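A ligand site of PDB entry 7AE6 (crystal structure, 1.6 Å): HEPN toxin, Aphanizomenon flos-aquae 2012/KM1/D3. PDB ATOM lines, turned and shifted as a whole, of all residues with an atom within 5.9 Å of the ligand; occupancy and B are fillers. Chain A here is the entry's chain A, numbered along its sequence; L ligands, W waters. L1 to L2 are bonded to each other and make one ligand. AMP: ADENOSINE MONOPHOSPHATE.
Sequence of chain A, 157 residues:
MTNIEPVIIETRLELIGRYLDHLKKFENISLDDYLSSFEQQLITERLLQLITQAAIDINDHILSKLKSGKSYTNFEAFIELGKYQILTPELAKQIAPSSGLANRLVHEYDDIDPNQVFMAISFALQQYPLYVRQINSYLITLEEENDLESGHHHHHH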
ATOM      1  N   THR A  73      -2.900  38.470  -4.576  1.00  0.00           N
ATOM      2  CA  THR A  73      -2.962  37.028  -4.419  1.00  0.00           C
ATOM      3  C   THR A  73      -2.687  36.355  -5.763  1.00  0.00           C
ATOM      4  O   THR A  73      -2.641  37.015  -6.819  1.00  0.00           O
ATOM      5  CB  THR A  73      -4.327  36.590  -3.894  1.00  0.00           C
ATOM      6  OG1 THR A  73      -5.320  36.811  -4.912  1.00  0.00           O
ATOM      7  CG2 THR A  73      -4.707  37.387  -2.648  1.00  0.00           C
ATOM      8  N   PHE A  75      -4.657  34.285  -7.382  1.00  0.00           N
ATOM      9  CA  PHE A  75      -5.847  34.476  -8.216  1.00  0.00           C
ATOM     10  C   PHE A  75      -5.832  35.861  -8.853  1.00  0.00           C
ATOM     11  O   PHE A  75      -6.039  36.022 -10.056  1.00  0.00           O
ATOM     12  CB  PHE A  75      -7.109  34.281  -7.382  1.00  0.00           C
ATOM     13  CG  PHE A  75      -8.403  34.355  -8.179  1.00  0.00           C
ATOM     14  CD1 PHE A  75      -8.933  35.575  -8.570  1.00  0.00           C
ATOM     15  CD2 PHE A  75      -9.093  33.189  -8.505  1.00  0.00           C
ATOM     16  CE1 PHE A  75     -10.126  35.637  -9.297  1.00  0.00           C
ATOM     17  CE2 PHE A  75     -10.286  33.249  -9.211  1.00  0.00           C
ATOM     18  CZ  PHE A  75     -10.794  34.469  -9.623  1.00  0.00           C
ATOM     19  N   GLU A  76      -5.606  36.900  -8.025  1.00  0.00           N
ATOM     20  CA  GLU A  76      -5.673  38.272  -8.514  1.00  0.00           C
ATOM     21  C   GLU A  76      -4.638  38.540  -9.605  1.00  0.00           C
ATOM     22  O   GLU A  76      -4.884  39.363 -10.507  1.00  0.00           O
ATOM     23  CB  GLU A  76      -5.487  39.237  -7.352  1.00  0.00           C
ATOM     24  CG  GLU A  76      -6.654  39.262  -6.372  1.00  0.00           C
ATOM     25  CD  GLU A  76      -6.340  40.043  -5.117  1.00  0.00           C
ATOM     26  OE1 GLU A  76      -5.134  40.250  -4.845  1.00  0.00           O
ATOM     27  OE2 GLU A  76      -7.291  40.464  -4.414  1.00  0.00           O
ATOM     28  N   ALA A  96      -7.911  32.085 -13.984  1.00  0.00           N
ATOM     29  CA  ALA A  96      -7.621  32.490 -12.609  1.00  0.00           C
ATOM     30  C   ALA A  96      -7.943  31.433 -11.550  1.00  0.00           C
ATOM     31  O   ALA A  96      -7.147  31.261 -10.620  1.00  0.00           O
ATOM     32  CB  ALA A  96      -8.342  33.802 -12.280  1.00  0.00           C
ATOM     33  N   PRO A  97      -9.069  30.705 -11.615  1.00  0.00           N
ATOM     34  CA  PRO A  97      -9.334  29.686 -10.581  1.00  0.00           C
ATOM     35  C   PRO A  97      -8.293  28.580 -10.521  1.00  0.00           C
ATOM     36  O   PRO A  97      -8.270  27.828  -9.544  1.00  0.00           O
ATOM     37  CB  PRO A  97     -10.715  29.140 -10.962  1.00  0.00           C
ATOM     38  CG  PRO A  97     -11.349  30.222 -11.753  1.00  0.00           C
ATOM     39  CD  PRO A  97     -10.225  30.860 -12.522  1.00  0.00           C
ATOM     40  N   SER A  98      -7.432  28.440 -11.528  1.00  0.00           N
ATOM     41  CA  SER A  98      -6.383  27.439 -11.406  1.00  0.00           C
ATOM     42  C   SER A  98      -5.459  27.727 -10.234  1.00  0.00           C
ATOM     43  O   SER A  98      -4.815  26.801  -9.729  1.00  0.00           O
ATOM     44  CB  SER A  98      -5.596  27.298 -12.726  1.00  0.00           C
ATOM     45  OG  SER A  98      -4.784  28.423 -12.996  1.00  0.00           O
ATOM     46  N   SER A  99      -5.400  28.980  -9.758  1.00  0.00           N
ATOM     47  CA  SER A  99      -4.704  29.293  -8.517  1.00  0.00           C
ATOM     48  C   SER A  99      -5.310  28.549  -7.339  1.00  0.00           C
ATOM     49  O   SER A  99      -4.590  28.119  -6.427  1.00  0.00           O
ATOM     50  CB  SER A  99      -4.734  30.804  -8.277  1.00  0.00           C
ATOM     51  OG  SER A  99      -6.080  31.236  -8.121  1.00  0.00           O
ATOM     52  N   GLY A 100      -6.632  28.414  -7.304  1.00  0.00           N
ATOM     53  CA  GLY A 100      -7.252  27.655  -6.227  1.00  0.00           C
ATOM     54  C   GLY A 100      -6.960  26.180  -6.339  1.00  0.00           C
ATOM     55  O   GLY A 100      -6.738  25.502  -5.332  1.00  0.00           O
ATOM     56  N   LEU A 101      -6.965  25.653  -7.562  1.00  0.00           N
ATOM     57  CA  LEU A 101      -6.525  24.277  -7.792  1.00  0.00           C
ATOM     58  C   LEU A 101      -5.106  24.064  -7.259  1.00  0.00           C
ATOM     59  O   LEU A 101      -4.844  23.089  -6.544  1.00  0.00           O
ATOM     60  CB  LEU A 101      -6.595  23.974  -9.284  1.00  0.00           C
ATOM     61  CG  LEU A 101      -6.078  22.586  -9.705  1.00  0.00           C
ATOM     62  CD1 LEU A 101      -6.956  21.499  -9.110  1.00  0.00           C
ATOM     63  CD2 LEU A 101      -6.033  22.511 -11.230  1.00  0.00           C
ATOM     64  N   ASN A 103      -3.488  25.690  -4.938  1.00  0.00           N
ATOM     65  CA  ASN A 103      -3.455  25.725  -3.486  1.00  0.00           C
ATOM     66  C   ASN A 103      -3.943  24.412  -2.899  1.00  0.00           C
ATOM     67  O   ASN A 103      -3.409  23.921  -1.906  1.00  0.00           O
ATOM     68  CB  ASN A 103      -4.287  26.893  -2.952  1.00  0.00           C
ATOM     69  CG  ASN A 103      -3.605  28.243  -3.150  1.00  0.00           C
ATOM     70  OD1 ASN A 103      -2.404  28.310  -3.375  1.00  0.00           O
ATOM     71  ND2 ASN A 103      -4.384  29.321  -3.038  1.00  0.00           N
ATOM     72  N   ARG A 104      -4.969  23.817  -3.521  1.00  0.00           N
ATOM     73  CA  ARG A 104      -5.468  22.532  -3.022  1.00  0.00           C
ATOM     74  C   ARG A 104      -4.457  21.419  -3.245  1.00  0.00           C
ATOM     75  O   ARG A 104      -4.320  20.518  -2.403  1.00  0.00           O
ATOM     76  CB  ARG A 104      -6.792  22.162  -3.696  1.00  0.00           C
ATOM     77  CG  ARG A 104      -7.967  23.005  -3.223  1.00  0.00           C
ATOM     78  CD  ARG A 104      -9.192  22.734  -4.056  1.00  0.00           C
ATOM     79  NE  ARG A 104     -10.192  23.797  -3.959  1.00  0.00           N
ATOM     80  CZ  ARG A 104     -11.200  23.786  -3.111  1.00  0.00           C
ATOM     81  NH1 ARG A 104     -11.352  22.758  -2.287  1.00  0.00           N
ATOM     82  NH2 ARG A 104     -12.069  24.801  -3.087  1.00  0.00           N
ATOM     83  N   TYR A 109      -5.274  23.880   1.922  1.00  0.00           N
ATOM     84  CA  TYR A 109      -6.562  23.618   2.557  1.00  0.00           C
ATOM     85  C   TYR A 109      -7.322  22.548   1.778  1.00  0.00           C
ATOM     86  O   TYR A 109      -6.993  22.255   0.625  1.00  0.00           O
ATOM     87  CB  TYR A 109      -7.410  24.892   2.669  1.00  0.00           C
ATOM     88  CG  TYR A 109      -7.663  25.602   1.342  1.00  0.00           C
ATOM     89  CD1 TYR A 109      -8.783  25.307   0.569  1.00  0.00           C
ATOM     90  CD2 TYR A 109      -6.792  26.572   0.876  1.00  0.00           C
ATOM     91  CE1 TYR A 109      -9.025  25.949  -0.634  1.00  0.00           C
ATOM     92  CE2 TYR A 109      -7.024  27.231  -0.325  1.00  0.00           C
ATOM     93  CZ  TYR A 109      -8.132  26.913  -1.070  1.00  0.00           C
ATOM     94  OH  TYR A 109      -8.364  27.572  -2.271  1.00  0.00           O
ATOM     95  N   ASP A 110      -8.325  21.944   2.432  1.00  0.00           N
ATOM     96  CA  ASP A 110      -9.343  21.070   1.830  1.00  0.00           C
ATOM     97  C   ASP A 110      -8.845  19.666   1.437  1.00  0.00           C
ATOM     98  O   ASP A 110      -7.681  19.328   1.651  1.00  0.00           O
ATOM     99  CB  ASP A 110      -9.968  21.737   0.613  1.00  0.00           C
ATOM    100  N   ASP A 111      -9.746  18.848   0.863  1.00  0.00           N
ATOM    101  CA  ASP A 111      -9.435  17.511   0.374  1.00  0.00           C
ATOM    102  C   ASP A 111      -9.721  17.411  -1.120  1.00  0.00           C
ATOM    103  O   ASP A 111     -10.605  18.098  -1.644  1.00  0.00           O
ATOM    104  CB  ASP A 111     -10.255  16.431   1.111  1.00  0.00           C
ATOM    105  CG  ASP A 111      -9.938  16.372   2.588  1.00  0.00           C
ATOM    106  OD1 ASP A 111      -8.866  16.869   2.990  1.00  0.00           O
ATOM    107  OD2 ASP A 111     -10.771  15.828   3.342  1.00  0.00           O
ATOM    108  N   ILE A 112      -8.988  16.534  -1.805  1.00  0.00           N
ATOM    109  CA  ILE A 112      -8.971  16.504  -3.266  1.00  0.00           C
ATOM    110  C   ILE A 112     -10.171  15.708  -3.772  1.00  0.00           C
ATOM    111  O   ILE A 112     -10.341  14.534  -3.427  1.00  0.00           O
ATOM    112  CB  ILE A 112      -7.663  15.905  -3.802  1.00  0.00           C
ATOM    113  CG1 ILE A 112      -6.481  16.797  -3.417  1.00  0.00           C
ATOM    114  CG2 ILE A 112      -7.738  15.751  -5.328  1.00  0.00           C
ATOM    115  CD1 ILE A 112      -6.494  18.158  -4.097  1.00  0.00           C
ATOM    116  N   ASP A 113     -10.987  16.342  -4.613  1.00  0.00           N
ATOM    117  CA  ASP A 113     -12.106  15.692  -5.283  1.00  0.00           C
ATOM    118  C   ASP A 113     -11.645  15.251  -6.670  1.00  0.00           C
ATOM    119  O   ASP A 113     -11.444  16.114  -7.541  1.00  0.00           O
ATOM    120  CB  ASP A 113     -13.285  16.651  -5.381  1.00  0.00           C
ATOM    121  CG  ASP A 113     -14.493  16.051  -6.108  1.00  0.00           C
ATOM    122  OD1 ASP A 113     -14.437  14.889  -6.552  1.00  0.00           O
ATOM    123  OD2 ASP A 113     -15.499  16.776  -6.228  1.00  0.00           O
ATOM    124  N   PRO A 114     -11.476  13.951  -6.927  1.00  0.00           N
ATOM    125  CA  PRO A 114     -10.973  13.535  -8.240  1.00  0.00           C
ATOM    126  C   PRO A 114     -11.882  13.944  -9.388  1.00  0.00           C
ATOM    127  O   PRO A 114     -11.402  14.110 -10.519  1.00  0.00           O
ATOM    128  CB  PRO A 114     -10.894  11.999  -8.120  1.00  0.00           C
ATOM    129  CG  PRO A 114     -11.155  11.686  -6.679  1.00  0.00           C
ATOM    130  CD  PRO A 114     -11.943  12.811  -6.120  1.00  0.00           C
ATOM    131  N   GLN A 116     -13.297  16.800  -9.650  1.00  0.00           N
ATOM    132  CA  GLN A 116     -12.904  18.167  -9.991  1.00  0.00           C
ATOM    133  C   GLN A 116     -11.565  18.173 -10.724  1.00  0.00           C
ATOM    134  O   GLN A 116     -11.365  18.961 -11.662  1.00  0.00           O
ATOM    135  CB  GLN A 116     -12.812  19.025  -8.732  1.00  0.00           C
ATOM    136  CG  GLN A 116     -14.157  19.304  -8.080  1.00  0.00           C
ATOM    137  CD  GLN A 116     -14.939  20.387  -8.802  1.00  0.00           C
ATOM    138  OE1 GLN A 116     -14.362  21.322  -9.347  1.00  0.00           O
ATOM    139  NE2 GLN A 116     -16.256  20.263  -8.796  1.00  0.00           N
ATOM    140  N   VAL A 117     -10.632  17.304 -10.308  1.00  0.00           N
ATOM    141  CA  VAL A 117      -9.365  17.210 -11.022  1.00  0.00           C
ATOM    142  C   VAL A 117      -9.573  16.712 -12.436  1.00  0.00           C
ATOM    143  O   VAL A 117      -8.946  17.203 -13.380  1.00  0.00           O
ATOM    144  CB  VAL A 117      -8.383  16.317 -10.247  1.00  0.00           C
ATOM    145  CG1 VAL A 117      -7.035  16.281 -10.973  1.00  0.00           C
ATOM    146  CG2 VAL A 117      -8.207  16.859  -8.838  1.00  0.00           C
ATOM    147  N   ALA A 120     -10.535  19.530 -14.455  1.00  0.00           N
ATOM    148  CA  ALA A 120      -9.413  20.461 -14.600  1.00  0.00           C
ATOM    149  C   ALA A 120      -8.442  20.026 -15.687  1.00  0.00           C
ATOM    150  O   ALA A 120      -7.751  20.862 -16.281  1.00  0.00           O
ATOM    151  CB  ALA A 120      -8.685  20.627 -13.273  1.00  0.00           C
ATOM    152  N   PHE A 123      -9.979  21.597 -18.752  1.00  0.00           N
ATOM    153  CA  PHE A 123      -9.836  23.057 -18.675  1.00  0.00           C
ATOM    154  C   PHE A 123      -8.393  23.485 -18.919  1.00  0.00           C
ATOM    155  O   PHE A 123      -8.142  24.474 -19.624  1.00  0.00           O
ATOM    156  CB  PHE A 123     -10.305  23.564 -17.312  1.00  0.00           C
ATOM    157  CG  PHE A 123     -11.794  23.486 -17.092  1.00  0.00           C
ATOM    158  CD1 PHE A 123     -12.678  23.885 -18.090  1.00  0.00           C
ATOM    159  CD2 PHE A 123     -12.305  23.013 -15.903  1.00  0.00           C
ATOM    160  CE1 PHE A 123     -14.037  23.812 -17.888  1.00  0.00           C
ATOM    161  CE2 PHE A 123     -13.673  22.944 -15.691  1.00  0.00           C
ATOM    162  CZ  PHE A 123     -14.534  23.341 -16.688  1.00  0.00           C
HETATM  163  P   AMP L   1      -8.271  29.161  -2.433  1.00  0.00           P
HETATM  164  O1P AMP L   1      -6.981  29.492  -3.161  1.00  0.00           O
HETATM  165  O2P AMP L   1      -8.635  29.846  -1.129  1.00  0.00           O
HETATM  166  O5' AMP L   1      -9.473  29.310  -3.452  1.00  0.00           O
HETATM  167  C5' AMP L   1     -10.837  29.247  -3.007  1.00  0.00           C
HETATM  168  C4' AMP L   1     -11.762  29.570  -4.154  1.00  0.00           C
HETATM  169  O4' AMP L   1     -11.898  31.012  -4.275  1.00  0.00           O
HETATM  170  C3' AMP L   1     -11.249  29.059  -5.508  1.00  0.00           C
HETATM  171  O3' AMP L   1     -12.343  28.634  -6.315  1.00  0.00           O
HETATM  172  C2' AMP L   1     -10.621  30.313  -6.119  1.00  0.00           C
HETATM  173  O2' AMP L   1     -10.576  30.307  -7.527  1.00  0.00           O
HETATM  174  C1' AMP L   1     -11.559  31.406  -5.596  1.00  0.00           C
HETATM  175  N9  AMP L   1     -10.977  32.762  -5.533  1.00  0.00           N
HETATM  176  C8  AMP L   1      -9.782  33.124  -5.012  1.00  0.00           C
HETATM  177  N7  AMP L   1      -9.607  34.479  -5.117  1.00  0.00           N
HETATM  178  C5  AMP L   1     -10.695  34.992  -5.714  1.00  0.00           C
HETATM  179  C6  AMP L   1     -11.152  36.336  -6.141  1.00  0.00           C
HETATM  180  N6  AMP L   1     -10.402  37.458  -5.950  1.00  0.00           N
HETATM  181  N1  AMP L   1     -12.365  36.432  -6.744  1.00  0.00           N
HETATM  182  C2  AMP L   1     -13.130  35.345  -6.942  1.00  0.00           C
HETATM  183  N3  AMP L   1     -12.767  34.102  -6.585  1.00  0.00           N
HETATM  184  C4  AMP L   1     -11.584  33.861  -5.989  1.00  0.00           C
HETATM  185  P   AMP L   2     -12.855  27.112  -6.244  1.00  0.00           P
HETATM  186  O1P AMP L   2     -13.100  26.729  -4.800  1.00  0.00           O
HETATM  187  O2P AMP L   2     -14.008  26.990  -7.220  1.00  0.00           O
HETATM  188  O5' AMP L   2     -11.637  26.250  -6.788  1.00  0.00           O
HETATM  189  C5' AMP L   2     -10.930  26.602  -7.967  1.00  0.00           C
HETATM  190  C4' AMP L   2     -10.669  25.388  -8.846  1.00  0.00           C
HETATM  191  O4' AMP L   2     -10.101  24.331  -8.034  1.00  0.00           O
HETATM  192  C3' AMP L   2     -11.902  24.780  -9.483  1.00  0.00           C
HETATM  193  O3' AMP L   2     -12.248  25.406 -10.710  1.00  0.00           O
HETATM  194  C2' AMP L   2     -11.542  23.304  -9.645  1.00  0.00           C
HETATM  195  O2' AMP L   2     -10.797  23.102 -10.831  1.00  0.00           O
HETATM  196  C1' AMP L   2     -10.613  23.079  -8.447  1.00  0.00           C
HETATM  197  N9  AMP L   2     -11.302  22.470  -7.285  1.00  0.00           N
HETATM  198  C8  AMP L   2     -12.386  22.907  -6.633  1.00  0.00           C
HETATM  199  N7  AMP L   2     -12.694  22.068  -5.600  1.00  0.00           N
HETATM  200  C5  AMP L   2     -11.768  21.087  -5.599  1.00  0.00           C
HETATM  201  C6  AMP L   2     -11.486  19.888  -4.787  1.00  0.00           C
HETATM  202  N6  AMP L   2     -12.271  19.553  -3.739  1.00  0.00           N
HETATM  203  N1  AMP L   2     -10.412  19.139  -5.131  1.00  0.00           N
HETATM  204  C2  AMP L   2      -9.620  19.444  -6.162  1.00  0.00           C
HETATM  205  N3  AMP L   2      -9.810  20.524  -6.946  1.00  0.00           N
HETATM  206  C4  AMP L   2     -10.862  21.356  -6.713  1.00  0.00           C
HETATM  207  O   HOH W   1      -7.121  31.207  -5.315  1.00  0.00           O
HETATM  208  O   HOH W   2     -13.057  30.531  -8.830  1.00  0.00           O
HETATM  209  O   HOH W   3     -13.743  39.017  -6.481  1.00  0.00           O
HETATM  210  O   HOH W   4      -7.924  36.530  -4.359  1.00  0.00           O
HETATM  211  O   HOH W   5     -12.008  21.577 -12.310  1.00  0.00           O
HETATM  212  O   HOH W   6     -12.286  35.113  -2.608  1.00  0.00           O
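Water W5 lies within hydrogen-bond range of O2' of AMP L2 (2.4 Å), O of Gln 116 (2.8 Å) and N of Ala 120 (3.3 Å). Water W1 lies within hydrogen-bond range of O1P of AMP L1 (2.8 Å), OG of Ser 99 (3.0 Å) and N of Gly 100 (3.5 Å). Water W4 lies within hydrogen-bond range of OG1 of Thr 73 and N7 of AMP L1.
The side-chain hydroxyl of Tyr 109 is bonded to a phosphorus (P) of AMP L1. O1P of AMP L1 is in hydrogen-bond range of ND2 of Asn 103, at 2.6 Å. The guanidinium group (NH2) of Arg 104 lies within salt-bridge range of an oxygen (O1P) of AMP L2, 2.8 Å away. A nitrogen (N1) of AMP L2 is in hydrogen-bond range of the backbone NH (N) of Asp 113. The backbone carbonyl oxygen of Asp 111 is in hydrogen-bond range of a nitrogen (N6) of AMP L2, 3.0 Å away. O4' of AMP L2 is in hydrogen-bond range of N of Leu 101, 3.4 Å away.
OG of Ser 99 lies close to N of Phe 75.
Residues that only touch the ligand: Phe 75 (3.3 Å), Pro 97 (3.3 Å), Gly 100 (3.6 Å), Ile 112 (3.5 Å), Gln 116 (3.5 Å) and Val 117 (3.98 Å). Hydrophobic or aromatic side chains that line the ligand: Phe 75, Pro 97, Leu 101, Tyr 109, Ile 112 and Val 117. Within 4 Å of the ligand: Phe 75, Pro 97, Gly 100, Leu 101, Asn 103, Arg 104, Tyr 109, Asp 111, Ile 112, Asp 113, Gln 116 and Val 117.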
